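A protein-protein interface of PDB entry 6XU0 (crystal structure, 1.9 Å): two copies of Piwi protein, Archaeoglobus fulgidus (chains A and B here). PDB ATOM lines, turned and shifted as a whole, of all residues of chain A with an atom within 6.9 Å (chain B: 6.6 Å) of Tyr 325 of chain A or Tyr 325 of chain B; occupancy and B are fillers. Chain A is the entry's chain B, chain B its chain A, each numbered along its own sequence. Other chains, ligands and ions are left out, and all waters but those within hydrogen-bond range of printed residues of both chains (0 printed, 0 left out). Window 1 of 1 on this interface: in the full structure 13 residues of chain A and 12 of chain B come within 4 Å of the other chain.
Of chain B, only Tyr 325 (3.4 Å) and Thr 328 (3.2 Å) come within 4 Å of Tyr 325 of chain A.
Of the printed residues of chain B, Val 330 of chain A touches Phe 312 (3.7 Å).
Of the printed residues of chain A, Val 314 of chain B touches Lys 329 (3.7 Å).
Pro 324 of chain B touches none of the printed residues of chain A.
Tyr 325 of chain B touches two residues of chain A.
Phe 312 of chain A touches Val 330 of chain B, and with the chains exchanged Val 330 of chain A touches Phe 312 of chain B.
Val 314 of chain A touches Lys 329 of chain B, and with the chains exchanged Lys 329 of chain A touches Val 314 of chain B.
Tyr 325 of chain B touches its own counterpart, Tyr 325 of chain A.
Tyr 325 of chain A touches Thr 328 of chain B, and with the chains exchanged Thr 328 of chain A touches Tyr 325 of chain B.
Of the 7 pairs that touch across the chains among the printed residues, 7 have their exchanged pair printed and touching as well.
Val 330 of chain B touches Phe 312 of chain A (CG1 to CD1, 3.5 Å).
Val 314 of chain A touches Lys 329 of chain B (CA to O, 3.6 Å).
Tyr 325 of chain B touches Tyr 325 of chain A (CE1 to CE2, 3.4 Å).
Thr 328 of chain B touches Tyr 325 of chain A.
OH of Tyr 325 of chain B touches CG2 of Thr 328 of chain A (3.4 Å).
Val 314 of chain B touches Lys 329 of chain A.
Phe 312 of chain B touches Val 330 of chain A.
Of the 16 printed residues of chain A, 6 touch a printed residue of chain B.
Of the 16 printed residues of chain B, 6 touch a printed residue of chain A.
Among the printed residues, 7 pairs touch across the chains.
Among the printed residues, no Asp or Glu carboxylate lies within 4 Å of a Lys or Arg side-chain nitrogen of the other chain.
OG1 of Thr 340 of chain B is in hydrogen-bond range of O of Tyr 325 of chain B (3.0 Å).
The backbone NH of Thr 340 of chain B is in hydrogen-bond range of the backbone carbonyl oxygen of Thr 328 of chain B (3.2 Å).
The backbone carbonyl oxygen (O) of Phe 312 of chain A is in hydrogen-bond range of the backbone NH (N) of Ile 357 of chain A.
O of Val 314 of chain A is in hydrogen-bond range of N of Thr 355 of chain A.
O of Tyr 325 of chain A sits at hydrogen-bond distance from OG1 of Thr 328 of chain A, 3.0 Å away.
The backbone carbonyl oxygen (O) of Tyr 325 of chain A lies within hydrogen-bond range of the side-chain hydroxyl (OG1) of Thr 340 of chain A, at 3.2 Å.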
ATOM      1  N   PHE A 312       7.409 -31.820   0.011  1.00  0.00           N
ATOM      2  CA  PHE A 312       6.338 -32.478  -0.729  1.00  0.00           C
ATOM      3  C   PHE A 312       6.861 -32.973  -2.061  1.00  0.00           C
ATOM      4  O   PHE A 312       7.986 -32.675  -2.460  1.00  0.00           O
ATOM      5  CB  PHE A 312       5.113 -31.566  -0.958  1.00  0.00           C
ATOM      6  CG  PHE A 312       5.421 -30.254  -1.641  1.00  0.00           C
ATOM      7  CD1 PHE A 312       5.400 -30.144  -3.024  1.00  0.00           C
ATOM      8  CD2 PHE A 312       5.701 -29.118  -0.887  1.00  0.00           C
ATOM      9  CE1 PHE A 312       5.668 -28.938  -3.652  1.00  0.00           C
ATOM     10  CE2 PHE A 312       5.959 -27.921  -1.503  1.00  0.00           C
ATOM     11  CZ  PHE A 312       5.940 -27.835  -2.893  1.00  0.00           C
ATOM     12  N   VAL A 314       5.690 -33.525  -6.230  1.00  0.00           N
ATOM     13  CA  VAL A 314       4.810 -33.312  -7.366  1.00  0.00           C
ATOM     14  C   VAL A 314       4.676 -34.633  -8.111  1.00  0.00           C
ATOM     15  O   VAL A 314       5.682 -35.238  -8.505  1.00  0.00           O
ATOM     16  CB  VAL A 314       5.349 -32.202  -8.272  1.00  0.00           C
ATOM     17  CG1 VAL A 314       4.531 -32.120  -9.536  1.00  0.00           C
ATOM     18  CG2 VAL A 314       5.380 -30.859  -7.514  1.00  0.00           C
ATOM     19  N   PRO A 324       9.508 -28.383 -15.066  1.00  0.00           N
ATOM     20  CA  PRO A 324      10.273 -28.171 -13.836  1.00  0.00           C
ATOM     21  C   PRO A 324       9.700 -27.077 -12.934  1.00  0.00           C
ATOM     22  O   PRO A 324       9.044 -26.130 -13.384  1.00  0.00           O
ATOM     23  CB  PRO A 324      11.660 -27.762 -14.351  1.00  0.00           C
ATOM     24  CG  PRO A 324      11.756 -28.369 -15.710  1.00  0.00           C
ATOM     25  CD  PRO A 324      10.361 -28.300 -16.268  1.00  0.00           C
ATOM     26  N   TYR A 325       9.954 -27.238 -11.642  1.00  0.00           N
ATOM     27  CA  TYR A 325       9.776 -26.185 -10.651  1.00  0.00           C
ATOM     28  C   TYR A 325      11.070 -25.415 -10.399  1.00  0.00           C
ATOM     29  O   TYR A 325      11.102 -24.524  -9.537  1.00  0.00           O
ATOM     30  CB  TYR A 325       9.249 -26.798  -9.357  1.00  0.00           C
ATOM     31  CG  TYR A 325       7.821 -27.238  -9.503  1.00  0.00           C
ATOM     32  CD1 TYR A 325       7.465 -28.234 -10.411  1.00  0.00           C
ATOM     33  CD2 TYR A 325       6.823 -26.633  -8.760  1.00  0.00           C
ATOM     34  CE1 TYR A 325       6.151 -28.623 -10.565  1.00  0.00           C
ATOM     35  CE2 TYR A 325       5.503 -27.013  -8.899  1.00  0.00           C
ATOM     36  CZ  TYR A 325       5.168 -28.007  -9.800  1.00  0.00           C
ATOM     37  OH  TYR A 325       3.837 -28.361  -9.921  1.00  0.00           O
ATOM     38  N   GLU A 326      12.120 -25.735 -11.158  1.00  0.00           N
ATOM     39  CA  GLU A 326      13.454 -25.189 -10.966  1.00  0.00           C
ATOM     40  C   GLU A 326      13.429 -23.673 -11.088  1.00  0.00           C
ATOM     41  O   GLU A 326      13.229 -23.127 -12.178  1.00  0.00           O
ATOM     42  CB  GLU A 326      14.406 -25.812 -11.985  1.00  0.00           C
ATOM     43  CG  GLU A 326      15.841 -25.362 -11.822  1.00  0.00           C
ATOM     44  CD  GLU A 326      16.501 -25.789 -10.525  1.00  0.00           C
ATOM     45  OE1 GLU A 326      15.935 -26.649  -9.838  1.00  0.00           O
ATOM     46  OE2 GLU A 326      17.573 -25.253 -10.214  1.00  0.00           O
ATOM     47  N   GLY A 327      13.625 -22.984  -9.964  1.00  0.00           N
ATOM     48  CA  GLY A 327      13.542 -21.542  -9.943  1.00  0.00           C
ATOM     49  C   GLY A 327      12.155 -20.967  -9.734  1.00  0.00           C
ATOM     50  O   GLY A 327      11.983 -19.748  -9.865  1.00  0.00           O
ATOM     51  N   THR A 328      11.168 -21.784  -9.375  1.00  0.00           N
ATOM     52  CA  THR A 328       9.811 -21.281  -9.241  1.00  0.00           C
ATOM     53  C   THR A 328       9.629 -20.564  -7.910  1.00  0.00           C
ATOM     54  O   THR A 328      10.131 -21.007  -6.871  1.00  0.00           O
ATOM     55  CB  THR A 328       8.809 -22.423  -9.365  1.00  0.00           C
ATOM     56  OG1 THR A 328       8.843 -22.924 -10.699  1.00  0.00           O
ATOM     57  CG2 THR A 328       7.401 -21.945  -9.027  1.00  0.00           C
ATOM     58  N   LYS A 329       8.902 -19.453  -7.954  1.00  0.00           N
ATOM     59  CA  LYS A 329       8.613 -18.633  -6.790  1.00  0.00           C
ATOM     60  C   LYS A 329       7.101 -18.542  -6.593  1.00  0.00           C
ATOM     61  O   LYS A 329       6.359 -18.223  -7.530  1.00  0.00           O
ATOM     62  CB  LYS A 329       9.211 -17.240  -6.959  1.00  0.00           C
ATOM     63  CG  LYS A 329      10.646 -17.252  -7.498  1.00  0.00           C
ATOM     64  CD  LYS A 329      11.045 -15.858  -7.961  1.00  0.00           C
ATOM     65  CE  LYS A 329      11.319 -15.795  -9.460  1.00  0.00           C
ATOM     66  NZ  LYS A 329      11.716 -14.400  -9.840  1.00  0.00           N
ATOM     67  N   VAL A 330       6.655 -18.789  -5.369  1.00  0.00           N
ATOM     68  CA  VAL A 330       5.245 -18.713  -5.007  1.00  0.00           C
ATOM     69  C   VAL A 330       5.048 -17.560  -4.035  1.00  0.00           C
ATOM     70  O   VAL A 330       5.802 -17.416  -3.060  1.00  0.00           O
ATOM     71  CB  VAL A 330       4.759 -20.038  -4.405  1.00  0.00           C
ATOM     72  CG1 VAL A 330       3.456 -19.829  -3.682  1.00  0.00           C
ATOM     73  CG2 VAL A 330       4.637 -21.071  -5.497  1.00  0.00           C
ATOM     74  N   LEU A 339       9.886 -20.671  -2.078  1.00  0.00           N
ATOM     75  CA  LEU A 339      10.728 -21.145  -3.177  1.00  0.00           C
ATOM     76  C   LEU A 339      10.686 -22.661  -3.237  1.00  0.00           C
ATOM     77  O   LEU A 339      10.993 -23.330  -2.253  1.00  0.00           O
ATOM     78  CB  LEU A 339      12.179 -20.706  -3.005  1.00  0.00           C
ATOM     79  CG  LEU A 339      12.627 -19.340  -3.501  1.00  0.00           C
ATOM     80  CD1 LEU A 339      11.567 -18.290  -3.259  1.00  0.00           C
ATOM     81  CD2 LEU A 339      13.915 -18.986  -2.771  1.00  0.00           C
ATOM     82  N   THR A 340      10.336 -23.209  -4.404  1.00  0.00           N
ATOM     83  CA  THR A 340      10.257 -24.663  -4.560  1.00  0.00           C
ATOM     84  C   THR A 340      11.629 -25.170  -4.997  1.00  0.00           C
ATOM     85  O   THR A 340      11.886 -25.436  -6.173  1.00  0.00           O
ATOM     86  CB  THR A 340       9.167 -25.033  -5.571  1.00  0.00           C
ATOM     87  OG1 THR A 340       9.436 -24.380  -6.821  1.00  0.00           O
ATOM     88  CG2 THR A 340       7.787 -24.564  -5.065  1.00  0.00           C
ATOM     89  N   LEU A 341      12.538 -25.283  -4.028  1.00  0.00           N
ATOM     90  CA  LEU A 341      13.876 -25.792  -4.311  1.00  0.00           C
ATOM     91  C   LEU A 341      13.806 -27.294  -4.574  1.00  0.00           C
ATOM     92  O   LEU A 341      13.156 -28.035  -3.827  1.00  0.00           O
ATOM     93  CB  LEU A 341      14.824 -25.487  -3.139  1.00  0.00           C
ATOM     94  CG  LEU A 341      14.839 -24.007  -2.750  1.00  0.00           C
ATOM     95  CD1 LEU A 341      15.790 -23.754  -1.557  1.00  0.00           C
ATOM     96  CD2 LEU A 341      15.177 -23.090  -3.949  1.00  0.00           C
ATOM     97  N   LEU A 342      14.441 -27.745  -5.656  1.00  0.00           N
ATOM     98  CA  LEU A 342      14.351 -29.150  -6.048  1.00  0.00           C
ATOM     99  C   LEU A 342      15.383 -29.957  -5.285  1.00  0.00           C
ATOM    100  O   LEU A 342      16.583 -29.700  -5.407  1.00  0.00           O
ATOM    101  CB  LEU A 342      14.575 -29.321  -7.550  1.00  0.00           C
ATOM    102  CG  LEU A 342      13.615 -28.553  -8.454  1.00  0.00           C
ATOM    103  CD1 LEU A 342      13.777 -28.990  -9.912  1.00  0.00           C
ATOM    104  CD2 LEU A 342      12.200 -28.747  -7.983  1.00  0.00           C
ATOM    105  N   THR A 355       8.415 -35.769  -8.228  1.00  0.00           N
ATOM    106  CA  THR A 355       9.483 -34.787  -8.127  1.00  0.00           C
ATOM    107  C   THR A 355       9.551 -34.300  -6.686  1.00  0.00           C
ATOM    108  O   THR A 355       8.664 -33.546  -6.260  1.00  0.00           O
ATOM    109  CB  THR A 355       9.246 -33.606  -9.067  1.00  0.00           C
ATOM    110  OG1 THR A 355       9.186 -34.057 -10.423  1.00  0.00           O
ATOM    111  CG2 THR A 355      10.364 -32.583  -8.919  1.00  0.00           C
ATOM    112  N   ILE A 357      10.191 -31.967  -3.675  1.00  0.00           N
ATOM    113  CA  ILE A 357      10.403 -30.547  -3.447  1.00  0.00           C
ATOM    114  C   ILE A 357      10.784 -30.364  -1.985  1.00  0.00           C
ATOM    115  O   ILE A 357      10.209 -31.004  -1.097  1.00  0.00           O
ATOM    116  CB  ILE A 357       9.150 -29.711  -3.803  1.00  0.00           C
ATOM    117  CG1 ILE A 357       8.632 -30.104  -5.181  1.00  0.00           C
ATOM    118  CG2 ILE A 357       9.462 -28.223  -3.772  1.00  0.00           C
ATOM    119  CD1 ILE A 357       9.636 -29.941  -6.277  1.00  0.00           C
ATOM    120  N   TYR A 386      17.605 -18.247  -4.471  1.00  0.00           N
ATOM    121  CA  TYR A 386      17.755 -19.388  -5.351  1.00  0.00           C
ATOM    122  C   TYR A 386      19.220 -19.584  -5.769  1.00  0.00           C
ATOM    123  O   TYR A 386      19.740 -20.707  -5.733  1.00  0.00           O
ATOM    124  CB  TYR A 386      16.835 -19.194  -6.572  1.00  0.00           C
ATOM    125  CG  TYR A 386      17.013 -20.233  -7.634  1.00  0.00           C
ATOM    126  CD1 TYR A 386      16.645 -21.567  -7.415  1.00  0.00           C
ATOM    127  CD2 TYR A 386      17.561 -19.886  -8.869  1.00  0.00           C
ATOM    128  CE1 TYR A 386      16.830 -22.526  -8.413  1.00  0.00           C
ATOM    129  CE2 TYR A 386      17.743 -20.833  -9.862  1.00  0.00           C
ATOM    130  CZ  TYR A 386      17.379 -22.136  -9.632  1.00  0.00           C
ATOM    131  OH  TYR A 386      17.566 -23.049 -10.635  1.00  0.00           O
ATOM    132  N   PHE B 312      -2.969 -18.963  -3.493  1.00  0.00           N
ATOM    133  CA  PHE B 312      -1.616 -18.417  -3.641  1.00  0.00           C
ATOM    134  C   PHE B 312      -1.377 -18.106  -5.111  1.00  0.00           C
ATOM    135  O   PHE B 312      -2.197 -18.439  -5.966  1.00  0.00           O
ATOM    136  CB  PHE B 312      -0.534 -19.375  -3.086  1.00  0.00           C
ATOM    137  CG  PHE B 312      -0.503 -20.745  -3.746  1.00  0.00           C
ATOM    138  CD1 PHE B 312       0.178 -20.949  -4.917  1.00  0.00           C
ATOM    139  CD2 PHE B 312      -1.122 -21.844  -3.144  1.00  0.00           C
ATOM    140  CE1 PHE B 312       0.222 -22.198  -5.511  1.00  0.00           C
ATOM    141  CE2 PHE B 312      -1.071 -23.094  -3.730  1.00  0.00           C
ATOM    142  CZ  PHE B 312      -0.401 -23.261  -4.934  1.00  0.00           C
ATOM    143  N   VAL B 314       1.561 -17.976  -8.339  1.00  0.00           N
ATOM    144  CA  VAL B 314       2.871 -18.311  -8.874  1.00  0.00           C
ATOM    145  C   VAL B 314       3.421 -17.091  -9.606  1.00  0.00           C
ATOM    146  O   VAL B 314       2.679 -16.363 -10.285  1.00  0.00           O
ATOM    147  CB  VAL B 314       2.796 -19.548  -9.781  1.00  0.00           C
ATOM    148  CG1 VAL B 314       4.174 -19.913 -10.265  1.00  0.00           C
ATOM    149  CG2 VAL B 314       2.201 -20.691  -9.008  1.00  0.00           C
ATOM    150  N   PRO B 324       1.095 -24.945 -16.524  1.00  0.00           N
ATOM    151  CA  PRO B 324       2.023 -25.830 -15.799  1.00  0.00           C
ATOM    152  C   PRO B 324       1.390 -26.465 -14.561  1.00  0.00           C
ATOM    153  O   PRO B 324       1.755 -27.580 -14.180  1.00  0.00           O
ATOM    154  CB  PRO B 324       3.169 -24.894 -15.402  1.00  0.00           C
ATOM    155  CG  PRO B 324       3.137 -23.818 -16.443  1.00  0.00           C
ATOM    156  CD  PRO B 324       1.683 -23.618 -16.782  1.00  0.00           C
ATOM    157  N   TYR B 325       0.444 -25.759 -13.942  1.00  0.00           N
ATOM    158  CA  TYR B 325      -0.278 -26.262 -12.779  1.00  0.00           C
ATOM    159  C   TYR B 325      -1.700 -26.675 -13.104  1.00  0.00           C
ATOM    160  O   TYR B 325      -2.463 -26.991 -12.189  1.00  0.00           O
ATOM    161  CB  TYR B 325      -0.277 -25.214 -11.667  1.00  0.00           C
ATOM    162  CG  TYR B 325       1.117 -24.713 -11.464  1.00  0.00           C
ATOM    163  CD1 TYR B 325       2.033 -25.442 -10.714  1.00  0.00           C
ATOM    164  CD2 TYR B 325       1.542 -23.544 -12.077  1.00  0.00           C
ATOM    165  CE1 TYR B 325       3.321 -24.996 -10.562  1.00  0.00           C
ATOM    166  CE2 TYR B 325       2.824 -23.098 -11.934  1.00  0.00           C
ATOM    167  CZ  TYR B 325       3.709 -23.819 -11.181  1.00  0.00           C
ATOM    168  OH  TYR B 325       4.990 -23.341 -11.046  1.00  0.00           O
ATOM    169  N   GLU B 326      -2.079 -26.683 -14.373  1.00  0.00           N
ATOM    170  CA  GLU B 326      -3.399 -27.183 -14.728  1.00  0.00           C
ATOM    171  C   GLU B 326      -3.392 -28.696 -14.571  1.00  0.00           C
ATOM    172  O   GLU B 326      -2.693 -29.408 -15.303  1.00  0.00           O
ATOM    173  CB  GLU B 326      -3.781 -26.766 -16.146  1.00  0.00           C
ATOM    174  CG  GLU B 326      -5.199 -27.193 -16.578  1.00  0.00           C
ATOM    175  CD  GLU B 326      -6.340 -26.534 -15.787  1.00  0.00           C
ATOM    176  OE1 GLU B 326      -6.102 -25.549 -15.048  1.00  0.00           O
ATOM    177  OE2 GLU B 326      -7.493 -27.015 -15.920  1.00  0.00           O
ATOM    178  N   GLY B 327      -4.155 -29.185 -13.604  1.00  0.00           N
ATOM    179  CA  GLY B 327      -4.169 -30.602 -13.314  1.00  0.00           C
ATOM    180  C   GLY B 327      -2.962 -31.108 -12.541  1.00  0.00           C
ATOM    181  O   GLY B 327      -2.658 -32.304 -12.614  1.00  0.00           O
ATOM    182  N   THR B 328      -2.285 -30.247 -11.774  1.00  0.00           N
ATOM    183  CA  THR B 328      -1.096 -30.667 -11.040  1.00  0.00           C
ATOM    184  C   THR B 328      -1.487 -31.288  -9.698  1.00  0.00           C
ATOM    185  O   THR B 328      -2.361 -30.775  -8.984  1.00  0.00           O
ATOM    186  CB  THR B 328      -0.121 -29.505 -10.844  1.00  0.00           C
ATOM    187  OG1 THR B 328       0.465 -29.183 -12.112  1.00  0.00           O
ATOM    188  CG2 THR B 328       1.013 -29.895  -9.863  1.00  0.00           C
ATOM    189  N   LYS B 329      -0.869 -32.424  -9.392  1.00  0.00           N
ATOM    190  CA  LYS B 329      -1.130 -33.167  -8.164  1.00  0.00           C
ATOM    191  C   LYS B 329       0.118 -33.094  -7.281  1.00  0.00           C
ATOM    192  O   LYS B 329       1.237 -33.330  -7.756  1.00  0.00           O
ATOM    193  CB  LYS B 329      -1.518 -34.626  -8.482  1.00  0.00           C
ATOM    194  CG  LYS B 329      -2.719 -34.761  -9.407  1.00  0.00           C
ATOM    195  CD  LYS B 329      -3.093 -36.209  -9.750  1.00  0.00           C
ATOM    196  CE  LYS B 329      -1.969 -36.946 -10.455  1.00  0.00           C
ATOM    197  NZ  LYS B 329      -2.164 -37.046 -11.922  1.00  0.00           N
ATOM    198  N   VAL B 330      -0.064 -32.712  -6.026  1.00  0.00           N
ATOM    199  CA  VAL B 330       1.013 -32.585  -5.049  1.00  0.00           C
ATOM    200  C   VAL B 330       0.739 -33.591  -3.955  1.00  0.00           C
ATOM    201  O   VAL B 330      -0.383 -33.647  -3.442  1.00  0.00           O
ATOM    202  CB  VAL B 330       1.081 -31.177  -4.444  1.00  0.00           C
ATOM    203  CG1 VAL B 330       2.090 -31.109  -3.292  1.00  0.00           C
ATOM    204  CG2 VAL B 330       1.382 -30.149  -5.530  1.00  0.00           C
ATOM    205  N   LEU B 339      -4.556 -30.470  -4.885  1.00  0.00           N
ATOM    206  CA  LEU B 339      -4.840 -30.306  -6.304  1.00  0.00           C
ATOM    207  C   LEU B 339      -4.769 -28.802  -6.608  1.00  0.00           C
ATOM    208  O   LEU B 339      -5.491 -28.008  -5.995  1.00  0.00           O
ATOM    209  CB  LEU B 339      -6.237 -30.864  -6.600  1.00  0.00           C
ATOM    210  CG  LEU B 339      -6.355 -31.692  -7.879  1.00  0.00           C
ATOM    211  CD1 LEU B 339      -5.036 -32.374  -8.207  1.00  0.00           C
ATOM    212  CD2 LEU B 339      -7.471 -32.719  -7.757  1.00  0.00           C
ATOM    213  N   THR B 340      -3.876 -28.396  -7.508  1.00  0.00           N
ATOM    214  CA  THR B 340      -3.629 -26.968  -7.730  1.00  0.00           C
ATOM    215  C   THR B 340      -4.574 -26.545  -8.847  1.00  0.00           C
ATOM    216  O   THR B 340      -4.245 -26.607 -10.025  1.00  0.00           O
ATOM    217  CB  THR B 340      -2.161 -26.677  -8.071  1.00  0.00           C
ATOM    218  OG1 THR B 340      -1.804 -27.310  -9.303  1.00  0.00           O
ATOM    219  CG2 THR B 340      -1.243 -27.196  -6.985  1.00  0.00           C
ATOM    220  N   LEU B 341      -5.792 -26.165  -8.480  1.00  0.00           N
ATOM    221  CA  LEU B 341      -6.776 -25.772  -9.480  1.00  0.00           C
ATOM    222  C   LEU B 341      -6.548 -24.305  -9.843  1.00  0.00           C
ATOM    223  O   LEU B 341      -6.429 -23.448  -8.959  1.00  0.00           O
ATOM    224  CB  LEU B 341      -8.198 -26.000  -8.939  1.00  0.00           C
ATOM    225  CG  LEU B 341      -8.495 -27.422  -8.419  1.00  0.00           C
ATOM    226  CD1 LEU B 341      -9.794 -27.542  -7.625  1.00  0.00           C
ATOM    227  CD2 LEU B 341      -8.496 -28.444  -9.583  1.00  0.00           C
ATOM    228  N   LEU B 342      -6.435 -24.026 -11.140  1.00  0.00           N
ATOM    229  CA  LEU B 342      -6.313 -22.647 -11.595  1.00  0.00           C
ATOM    230  C   LEU B 342      -7.584 -21.853 -11.295  1.00  0.00           C
ATOM    231  O   LEU B 342      -8.700 -22.384 -11.313  1.00  0.00           O
ATOM    232  CB  LEU B 342      -6.029 -22.592 -13.098  1.00  0.00           C
ATOM    233  CG  LEU B 342      -4.614 -22.861 -13.598  1.00  0.00           C
ATOM    234  CD1 LEU B 342      -4.598 -22.783 -15.114  1.00  0.00           C
ATOM    235  CD2 LEU B 342      -3.618 -21.880 -13.013  1.00  0.00           C
ATOM    236  N   THR B 355       0.056 -15.853 -11.502  1.00  0.00           N
ATOM    237  CA  THR B 355      -0.975 -16.834 -11.844  1.00  0.00           C
ATOM    238  C   THR B 355      -1.727 -17.284 -10.590  1.00  0.00           C
ATOM    239  O   THR B 355      -1.159 -18.020  -9.762  1.00  0.00           O
ATOM    240  CB  THR B 355      -0.353 -18.041 -12.542  1.00  0.00           C
ATOM    241  OG1 THR B 355       0.290 -17.608 -13.744  1.00  0.00           O
ATOM    242  CG2 THR B 355      -1.414 -19.063 -12.884  1.00  0.00           C
ATOM    243  N   ILE B 357      -3.776 -19.427  -8.031  1.00  0.00           N
ATOM    244  CA  ILE B 357      -4.042 -20.839  -7.801  1.00  0.00           C
ATOM    245  C   ILE B 357      -5.048 -20.924  -6.671  1.00  0.00           C
ATOM    246  O   ILE B 357      -4.895 -20.242  -5.650  1.00  0.00           O
ATOM    247  CB  ILE B 357      -2.755 -21.611  -7.445  1.00  0.00           C
ATOM    248  CG1 ILE B 357      -1.671 -21.393  -8.511  1.00  0.00           C
ATOM    249  CG2 ILE B 357      -3.063 -23.119  -7.182  1.00  0.00           C
ATOM    250  CD1 ILE B 357      -2.019 -21.928  -9.890  1.00  0.00           C
ATOM    251  N   TYR B 386     -10.138 -33.660 -10.414  1.00  0.00           N
ATOM    252  CA  TYR B 386      -9.827 -32.610 -11.398  1.00  0.00           C
ATOM    253  C   TYR B 386     -10.878 -32.576 -12.515  1.00  0.00           C
ATOM    254  O   TYR B 386     -11.375 -31.500 -12.870  1.00  0.00           O
ATOM    255  CB  TYR B 386      -8.412 -32.800 -11.974  1.00  0.00           C
ATOM    256  CG  TYR B 386      -8.128 -31.920 -13.202  1.00  0.00           C
ATOM    257  CD1 TYR B 386      -7.906 -30.548 -13.069  1.00  0.00           C
ATOM    258  CD2 TYR B 386      -8.126 -32.462 -14.462  1.00  0.00           C
ATOM    259  CE1 TYR B 386      -7.656 -29.723 -14.212  1.00  0.00           C
ATOM    260  CE2 TYR B 386      -7.884 -31.670 -15.592  1.00  0.00           C
ATOM    261  CZ  TYR B 386      -7.646 -30.317 -15.447  1.00  0.00           C
ATOM    262  OH  TYR B 386      -7.411 -29.546 -16.546  1.00  0.00           O
